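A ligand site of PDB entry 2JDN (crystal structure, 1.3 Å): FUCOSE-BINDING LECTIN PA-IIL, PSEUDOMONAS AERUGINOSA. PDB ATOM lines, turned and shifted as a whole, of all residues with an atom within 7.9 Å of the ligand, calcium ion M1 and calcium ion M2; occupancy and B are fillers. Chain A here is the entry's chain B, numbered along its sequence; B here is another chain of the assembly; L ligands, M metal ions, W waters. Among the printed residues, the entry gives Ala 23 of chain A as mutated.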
ATOM      1  N   ALA A  21      -1.486 -20.105  28.039  1.00  0.00           N
ATOM      2  CA  ALA A  21      -2.555 -19.569  27.148  1.00  0.00           C
ATOM      3  C   ALA A  21      -2.615 -20.344  25.840  1.00  0.00           C
ATOM      4  O   ALA A  21      -1.563 -20.688  25.249  1.00  0.00           O
ATOM      5  CB  ALA A  21      -2.312 -18.080  26.871  1.00  0.00           C
ATOM      6  N   ASN A  22      -3.836 -20.626  25.379  1.00  0.00           N
ATOM      7  CA  ASN A  22      -4.093 -21.296  24.105  1.00  0.00           C
ATOM      8  C   ASN A  22      -5.399 -20.748  23.517  1.00  0.00           C
ATOM      9  O   ASN A  22      -6.444 -21.429  23.571  1.00  0.00           O
ATOM     10  CB  ASN A  22      -4.229 -22.809  24.298  1.00  0.00           C
ATOM     11  CG  ASN A  22      -2.925 -23.452  24.647  1.00  0.00           C
ATOM     12  OD1 ASN A  22      -2.061 -23.648  23.761  1.00  0.00           O
ATOM     13  ND2 ASN A  22      -2.750 -23.795  25.928  1.00  0.00           N
ATOM     14  N   ALA A  23      -5.350 -19.559  22.928  1.00  0.00           N
ATOM     15  CA  ALA A  23      -6.583 -18.852  22.552  1.00  0.00           C
ATOM     16  C   ALA A  23      -6.228 -17.644  21.724  1.00  0.00           C
ATOM     17  O   ALA A  23      -5.150 -17.070  21.871  1.00  0.00           O
ATOM     18  CB  ALA A  23      -7.318 -18.399  23.817  1.00  0.00           C
ATOM     19  N   SER A  24      -7.138 -17.238  20.852  1.00  0.00           N
ATOM     20  CA  SER A  24      -7.014 -15.972  20.122  1.00  0.00           C
ATOM     21  C   SER A  24      -7.184 -14.763  21.050  1.00  0.00           C
ATOM     22  O   SER A  24      -6.502 -13.747  20.876  1.00  0.00           O
ATOM     23  CB  SER A  24      -8.020 -15.911  18.970  1.00  0.00           C
ATOM     24  OG  SER A  24      -7.713 -16.877  17.996  1.00  0.00           O
ATOM     25  N   GLY A  25      -8.070 -14.876  22.042  1.00  0.00           N
ATOM     26  CA  GLY A  25      -8.323 -13.793  22.995  1.00  0.00           C
ATOM     27  C   GLY A  25      -7.206 -13.700  24.018  1.00  0.00           C
ATOM     28  O   GLY A  25      -6.607 -14.720  24.428  1.00  0.00           O
ATOM     29  N   THR A  26      -6.898 -12.478  24.447  1.00  0.00           N
ATOM     30  CA  THR A  26      -5.947 -12.257  25.520  1.00  0.00           C
ATOM     31  C   THR A  26      -6.545 -12.735  26.826  1.00  0.00           C
ATOM     32  O   THR A  26      -7.642 -12.315  27.201  1.00  0.00           O
ATOM     33  CB  THR A  26      -5.589 -10.762  25.621  1.00  0.00           C
ATOM     34  OG1 THR A  26      -5.025 -10.332  24.379  1.00  0.00           O
ATOM     35  CG2 THR A  26      -4.623 -10.514  26.775  1.00  0.00           C
ATOM     36  N   GLN A  27      -5.821 -13.596  27.535  1.00  0.00           N
ATOM     37  CA  GLN A  27      -6.304 -14.185  28.769  1.00  0.00           C
ATOM     38  C   GLN A  27      -5.817 -13.362  29.934  1.00  0.00           C
ATOM     39  O   GLN A  27      -4.668 -12.883  29.919  1.00  0.00           O
ATOM     40  CB  GLN A  27      -5.765 -15.608  28.908  1.00  0.00           C
ATOM     41  CG  GLN A  27      -6.109 -16.487  27.721  1.00  0.00           C
ATOM     42  CD  GLN A  27      -7.595 -16.717  27.586  1.00  0.00           C
ATOM     43  OE1 GLN A  27      -8.258 -17.157  28.543  1.00  0.00           O
ATOM     44  NE2 GLN A  27      -8.119 -16.489  26.403  1.00  0.00           N
ATOM     45  N   GLN A  44      -1.532 -13.342  25.311  1.00  0.00           N
ATOM     46  CA  GLN A  44      -2.138 -14.070  24.231  1.00  0.00           C
ATOM     47  C   GLN A  44      -1.125 -15.025  23.637  1.00  0.00           C
ATOM     48  O   GLN A  44       0.003 -14.632  23.302  1.00  0.00           O
ATOM     49  CB  GLN A  44      -2.627 -13.127  23.104  1.00  0.00           C
ATOM     50  CG  GLN A  44      -3.459 -13.808  22.008  1.00  0.00           C
ATOM     51  CD  GLN A  44      -2.643 -14.529  20.918  1.00  0.00           C
ATOM     52  OE1 GLN A  44      -1.590 -14.013  20.458  1.00  0.00           O
ATOM     53  NE2 GLN A  44      -3.074 -15.695  20.502  1.00  0.00           N
ATOM     54  N   SER A  45      -1.539 -16.278  23.472  1.00  0.00           N
ATOM     55  CA  SER A  45      -0.744 -17.295  22.798  1.00  0.00           C
ATOM     56  C   SER A  45      -1.701 -18.344  22.273  1.00  0.00           C
ATOM     57  O   SER A  45      -2.683 -18.634  22.942  1.00  0.00           O
ATOM     58  CB  SER A  45       0.189 -17.982  23.786  1.00  0.00           C
ATOM     59  OG  SER A  45       1.007 -18.949  23.131  1.00  0.00           O
ATOM     60  N   THR A  46      -1.366 -18.971  21.144  1.00  0.00           N
ATOM     61  CA  THR A  46      -2.020 -20.212  20.761  1.00  0.00           C
ATOM     62  C   THR A  46      -1.027 -21.382  20.812  1.00  0.00           C
ATOM     63  O   THR A  46      -1.290 -22.455  20.252  1.00  0.00           O
ATOM     64  CB  THR A  46      -2.638 -20.118  19.342  1.00  0.00           C
ATOM     65  OG1 THR A  46      -1.652 -19.601  18.436  1.00  0.00           O
ATOM     66  CG2 THR A  46      -3.863 -19.239  19.342  1.00  0.00           C
ATOM     67  N   VAL A  70     -11.519 -12.657  29.842  1.00  0.00           N
ATOM     68  CA  VAL A  70     -10.982 -12.074  28.627  1.00  0.00           C
ATOM     69  C   VAL A  70     -11.630 -10.694  28.487  1.00  0.00           C
ATOM     70  O   VAL A  70     -12.867 -10.587  28.335  1.00  0.00           O
ATOM     71  CB  VAL A  70     -11.302 -12.927  27.405  1.00  0.00           C
ATOM     72  CG1 VAL A  70     -10.844 -12.220  26.110  1.00  0.00           C
ATOM     73  CG2 VAL A  70     -10.679 -14.313  27.524  1.00  0.00           C
ATOM     74  N   SER A  95     -10.147 -23.525  31.341  1.00  0.00           N
ATOM     75  CA  SER A  95     -11.116 -22.463  31.174  1.00  0.00           C
ATOM     76  C   SER A  95     -11.475 -22.311  29.715  1.00  0.00           C
ATOM     77  O   SER A  95     -10.671 -22.585  28.818  1.00  0.00           O
ATOM     78  CB  SER A  95     -10.585 -21.160  31.724  1.00  0.00           C
ATOM     79  OG  SER A  95      -9.501 -20.633  30.970  1.00  0.00           O
ATOM     80  N   GLU A  96     -12.725 -21.894  29.486  1.00  0.00           N
ATOM     81  CA  GLU A  96     -13.288 -21.768  28.150  1.00  0.00           C
ATOM     82  C   GLU A  96     -13.841 -20.361  27.973  1.00  0.00           C
ATOM     83  O   GLU A  96     -14.721 -19.941  28.744  1.00  0.00           O
ATOM     84  CB  GLU A  96     -14.371 -22.826  27.898  1.00  0.00           C
ATOM     85  CG  GLU A  96     -15.037 -22.722  26.524  1.00  0.00           C
ATOM     86  CD  GLU A  96     -14.038 -22.760  25.397  1.00  0.00           C
ATOM     87  OE1 GLU A  96     -13.160 -23.689  25.367  1.00  0.00           O
ATOM     88  OE2 GLU A  96     -14.049 -21.881  24.508  1.00  0.00           O
ATOM     89  N   ASP A  97     -13.333 -19.644  26.965  1.00  0.00           N
ATOM     90  CA  ASP A  97     -13.761 -18.274  26.675  1.00  0.00           C
ATOM     91  C   ASP A  97     -14.719 -18.182  25.509  1.00  0.00           C
ATOM     92  O   ASP A  97     -15.123 -17.052  25.154  1.00  0.00           O
ATOM     93  CB  ASP A  97     -12.526 -17.386  26.440  1.00  0.00           C
ATOM     94  CG  ASP A  97     -11.816 -17.694  25.134  1.00  0.00           C
ATOM     95  OD1 ASP A  97     -12.297 -18.506  24.321  1.00  0.00           O
ATOM     96  OD2 ASP A  97     -10.738 -17.088  24.890  1.00  0.00           O
ATOM     97  N   GLY A  98     -15.104 -19.292  24.911  1.00  0.00           N
ATOM     98  CA  GLY A  98     -15.867 -19.247  23.665  1.00  0.00           C
ATOM     99  C   GLY A  98     -16.787 -20.452  23.543  1.00  0.00           C
ATOM    100  O   GLY A  98     -17.438 -20.847  24.525  1.00  0.00           O
ATOM    101  N   THR A  99     -16.823 -21.037  22.357  1.00  0.00           N
ATOM    102  CA  THR A  99     -17.840 -22.043  22.026  1.00  0.00           C
ATOM    103  C   THR A  99     -17.267 -23.400  21.701  1.00  0.00           C
ATOM    104  O   THR A  99     -18.032 -24.352  21.645  1.00  0.00           O
ATOM    105  CB  THR A  99     -18.684 -21.610  20.809  1.00  0.00           C
ATOM    106  OG1 THR A  99     -17.801 -21.317  19.731  1.00  0.00           O
ATOM    107  CG2 THR A  99     -19.507 -20.371  21.129  1.00  0.00           C
ATOM    108  N   ASP A 100     -15.948 -23.517  21.480  1.00  0.00           N
ATOM    109  CA  ASP A 100     -15.398 -24.791  21.005  1.00  0.00           C
ATOM    110  C   ASP A 100     -15.189 -25.831  22.118  1.00  0.00           C
ATOM    111  O   ASP A 100     -14.983 -26.997  21.837  1.00  0.00           O
ATOM    112  CB  ASP A 100     -14.113 -24.631  20.162  1.00  0.00           C
ATOM    113  CG  ASP A 100     -12.940 -24.107  20.956  1.00  0.00           C
ATOM    114  OD1 ASP A 100     -13.107 -23.622  22.112  1.00  0.00           O
ATOM    115  OD2 ASP A 100     -11.807 -24.156  20.433  1.00  0.00           O
ATOM    116  N   ASN A 101     -15.226 -25.388  23.368  1.00  0.00           N
ATOM    117  CA  ASN A 101     -15.092 -26.284  24.521  1.00  0.00           C
ATOM    118  C   ASN A 101     -13.803 -27.077  24.529  1.00  0.00           C
ATOM    119  O   ASN A 101     -13.791 -28.225  24.987  1.00  0.00           O
ATOM    120  CB  ASN A 101     -16.349 -27.161  24.721  1.00  0.00           C
ATOM    121  CG  ASN A 101     -17.531 -26.348  25.138  1.00  0.00           C
ATOM    122  OD1 ASN A 101     -17.398 -25.227  25.624  1.00  0.00           O
ATOM    123  ND2 ASN A 101     -18.725 -26.918  24.946  1.00  0.00           N
ATOM    124  N   ASP A 102     -12.703 -26.479  24.075  1.00  0.00           N
ATOM    125  CA  ASP A 102     -11.422 -27.113  24.335  1.00  0.00           C
ATOM    126  C   ASP A 102     -10.941 -26.910  25.771  1.00  0.00           C
ATOM    127  O   ASP A 102     -10.095 -27.679  26.260  1.00  0.00           O
ATOM    128  CB  ASP A 102     -10.344 -26.780  23.261  1.00  0.00           C
ATOM    129  CG  ASP A 102      -9.981 -25.298  23.148  1.00  0.00           C
ATOM    130  OD1 ASP A 102     -10.570 -24.449  23.855  1.00  0.00           O
ATOM    131  OD2 ASP A 102      -9.065 -24.979  22.353  1.00  0.00           O
ATOM    132  N   TYR A 103     -11.481 -25.903  26.478  1.00  0.00           N
ATOM    133  CA  TYR A 103     -11.145 -25.668  27.882  1.00  0.00           C
ATOM    134  C   TYR A 103      -9.654 -25.473  28.150  1.00  0.00           C
ATOM    135  O   TYR A 103      -9.198 -25.642  29.274  1.00  0.00           O
ATOM    136  CB  TYR A 103     -11.778 -26.759  28.793  1.00  0.00           C
ATOM    137  CG  TYR A 103     -13.207 -26.359  29.108  1.00  0.00           C
ATOM    138  CD1 TYR A 103     -14.255 -26.717  28.255  1.00  0.00           C
ATOM    139  CD2 TYR A 103     -13.514 -25.549  30.213  1.00  0.00           C
ATOM    140  CE1 TYR A 103     -15.565 -26.263  28.498  1.00  0.00           C
ATOM    141  CE2 TYR A 103     -14.828 -25.113  30.469  1.00  0.00           C
ATOM    142  CZ  TYR A 103     -15.818 -25.487  29.601  1.00  0.00           C
ATOM    143  OH  TYR A 103     -17.113 -25.048  29.815  1.00  0.00           O
ATOM    144  N   ASN A 104      -8.911 -25.052  27.122  1.00  0.00           N
ATOM    145  CA  ASN A 104      -7.485 -24.822  27.287  1.00  0.00           C
ATOM    146  C   ASN A 104      -7.116 -23.348  27.116  1.00  0.00           C
ATOM    147  O   ASN A 104      -5.921 -23.024  27.009  1.00  0.00           O
ATOM    148  CB  ASN A 104      -6.688 -25.679  26.291  1.00  0.00           C
ATOM    149  CG  ASN A 104      -6.813 -25.142  24.887  1.00  0.00           C
ATOM    150  OD1 ASN A 104      -7.541 -24.167  24.653  1.00  0.00           O
ATOM    151  ND2 ASN A 104      -6.096 -25.756  23.962  1.00  0.00           N
ATOM    152  N   ASP A 105      -8.108 -22.453  27.125  1.00  0.00           N
ATOM    153  CA  ASP A 105      -7.843 -21.101  26.656  1.00  0.00           C
ATOM    154  C   ASP A 105      -6.893 -20.414  27.626  1.00  0.00           C
ATOM    155  O   ASP A 105      -5.919 -19.764  27.208  1.00  0.00           O
ATOM    156  CB  ASP A 105      -9.181 -20.367  26.473  1.00  0.00           C
ATOM    157  CG  ASP A 105     -10.032 -21.028  25.420  1.00  0.00           C
ATOM    158  OD1 ASP A 105      -9.509 -21.516  24.404  1.00  0.00           O
ATOM    159  OD2 ASP A 105     -11.263 -21.081  25.607  1.00  0.00           O
ATOM    160  N   ALA A 106      -7.151 -20.579  28.928  1.00  0.00           N
ATOM    161  CA  ALA A 106      -6.105 -20.434  29.949  1.00  0.00           C
ATOM    162  C   ALA A 106      -6.145 -21.712  30.772  1.00  0.00           C
ATOM    163  O   ALA A 106      -7.212 -22.154  31.191  1.00  0.00           O
ATOM    164  CB  ALA A 106      -6.354 -19.210  30.848  1.00  0.00           C
ATOM    165  N   PRO B 113      -5.025 -30.696  24.470  1.00  0.00           N
ATOM    166  CA  PRO B 113      -4.479 -30.118  23.251  1.00  0.00           C
ATOM    167  C   PRO B 113      -4.117 -28.663  23.463  1.00  0.00           C
ATOM    168  O   PRO B 113      -4.490 -28.011  24.453  1.00  0.00           O
ATOM    169  CB  PRO B 113      -5.647 -30.247  22.266  1.00  0.00           C
ATOM    170  CG  PRO B 113      -6.817 -30.105  23.081  1.00  0.00           C
ATOM    171  CD  PRO B 113      -6.490 -30.815  24.408  1.00  0.00           C
ATOM    172  N   LEU B 114      -3.379 -28.136  22.487  1.00  0.00           N
ATOM    173  CA  LEU B 114      -2.983 -26.735  22.463  1.00  0.00           C
ATOM    174  C   LEU B 114      -3.844 -25.993  21.460  1.00  0.00           C
ATOM    175  O   LEU B 114      -4.697 -26.584  20.804  1.00  0.00           O
ATOM    176  CB  LEU B 114      -1.498 -26.612  22.104  1.00  0.00           C
ATOM    177  CG  LEU B 114      -0.533 -27.383  22.992  1.00  0.00           C
ATOM    178  CD1 LEU B 114       0.889 -27.011  22.628  1.00  0.00           C
ATOM    179  CD2 LEU B 114      -0.822 -27.182  24.490  1.00  0.00           C
ATOM    180  N   GLY B 115      -3.616 -24.690  21.345  1.00  0.00           N
ATOM    181  CA  GLY B 115      -4.298 -23.890  20.342  1.00  0.00           C
ATOM    182  C   GLY B 115      -5.632 -23.279  20.721  1.00  0.00           C
ATOM    183  O   GLY B 115      -6.337 -23.730  21.654  1.00  0.00           O
ATOM    184  OXT GLY B 115      -5.990 -22.281  20.060  1.00  0.00           O
HETATM  185  C1  LIG L   1      -9.200 -19.864  19.247  1.00  0.00           C
HETATM  186  C2  LIG L   1      -9.215 -21.188  20.016  1.00  0.00           C
HETATM  187  C3  LIG L   1     -10.470 -21.293  20.863  1.00  0.00           C
HETATM  188  C4  LIG L   1     -10.708 -20.076  21.713  1.00  0.00           C
HETATM  189  C5  LIG L   1     -10.781 -18.874  20.759  1.00  0.00           C
HETATM  190  C6  LIG L   1     -11.035 -17.556  21.455  1.00  0.00           C
HETATM  191  C7  LIG L   1     -10.083 -18.968  17.256  1.00  0.00           C
HETATM  192  O1  LIG L   1     -10.159 -20.048  18.219  1.00  0.00           O
HETATM  193  O2  LIG L   1      -8.124 -21.234  20.936  1.00  0.00           O
HETATM  194  O3  LIG L   1     -10.388 -22.454  21.732  1.00  0.00           O
HETATM  195  O4  LIG L   1     -11.935 -20.266  22.451  1.00  0.00           O
HETATM  196  O5  LIG L   1      -9.518 -18.775  20.075  1.00  0.00           O
HETATM  197  O6  LIG L   1      -9.950 -17.188  22.322  1.00  0.00           O
HETATM  198 CA    CA M   1      -8.203 -22.804  22.885  1.00  0.00          CA
HETATM  199 CA    CA M   2     -11.842 -22.457  23.716  1.00  0.00          CA
HETATM  200  O   HOH W   1     -11.581 -22.956  17.388  1.00  0.00           O
HETATM  201  O   HOH W   2     -14.317 -20.809  20.853  1.00  0.00           O
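O6 of the ligand lies within hydrogen-bond range of OD2 of Asp 97 (2.7 Å). An oxygen (O5) of the ligand sits at hydrogen-bond distance from the backbone NH (N) of Ser 24, 2.9 Å away. An oxygen (O5) of the ligand sits close to the side-chain hydroxyl of Ser 24 (3.3 Å). The backbone NH (N) of Gly 25 sits at hydrogen-bond distance from an oxygen (O6) of the ligand, 3.0 Å away.
The backbone carbonyl oxygen of Ser 95 lies within hydrogen-bond range of the backbone NH of Asn 104 (3.5 Å). O of Pro 113 of chain B sits at hydrogen-bond distance from ND2 of Asn 104 (2.8 Å). N of Asn 22 lies close to O of Ser 45 (3.4 Å). OE2 of Glu 96 lies close to N of Gly 98. The backbone NH of Tyr 103 sits close to the side-chain carboxylate of Glu 96. The backbone carbonyl oxygen of Thr 46 sits close to the backbone NH of Gly 115 of chain B. OD2 of Asp 97 lies within hydrogen-bond range of NE2 of Gln 27 (3.1 Å). NE2 of Gln 27 is in hydrogen-bond range of O of Gly 25 (3.1 Å).
Residues that only touch the ligand: Ala 23 (3.3 Å). Hydrophobic or aromatic side chains within 4 Å of the ligand: Ala 23. Within 4 Å of the ligand: Asn 22, Ala 23, Ser 24, Gly 25, Glu 96, Asp 97, Asp 100, Asp 102, Asp 105 and Gly 115 of chain B. The nearest printed residue that does not touch the ligand is Gly 98 (4.1 Å).
Within 4 Å of calcium ion M1: Asn 22, Asp 102, Asn 104, Asp 105 and Gly 115 of chain B. The nearest printed residue that does not touch calcium ion M1 is Ala 23 (4.3 Å).
Calcium ion M1 is bound by OD1 of Asn 104, 2.3 Å away. The backbone carbonyl oxygen (O) of Asn 22 binds calcium ion M1. The side-chain carboxylate (OD1) of Asp 105 is bound to calcium ion M1, 2.4 Å away. OD2 of Asp 102 binds calcium ion M1 (2.4 Å). The chain-end carboxylate (O) of Gly 115 of chain B binds calcium ion M1 (2.4 Å). Calcium ion M1 is bound by O3 of the ligand (2.5 Å). Calcium ion M1 is bound by O2 of the ligand (2.5 Å). Calcium ion M1 has seven donor atoms within binding distance. Slightly farther from calcium ion M1 lies OD1 of Asp 102 (3.0 Å).
OD1 of Asp 100 binds calcium ion M2 (2.4 Å). Calcium ion M2 is bound by OD1 of Asp 102 (2.4 Å). Calcium ion M2 is bound by OD2 of Asp 105 (2.4 Å). OE2 of Glu 96 binds calcium ion M2, 2.4 Å away. The side-chain carboxylate (OE1) of Glu 96 binds calcium ion M2, 2.4 Å away. O3 of the ligand is bound to calcium ion M2, 2.5 Å away. O4 of the ligand binds calcium ion M2 (2.5 Å). The side-chain carboxylate (OD1) of Asp 105 is bound to calcium ion M2 (2.6 Å).
Water W1 bridges OD2 of Asp 100 (3.3 Å) and O1 of the ligand (3.3 Å).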
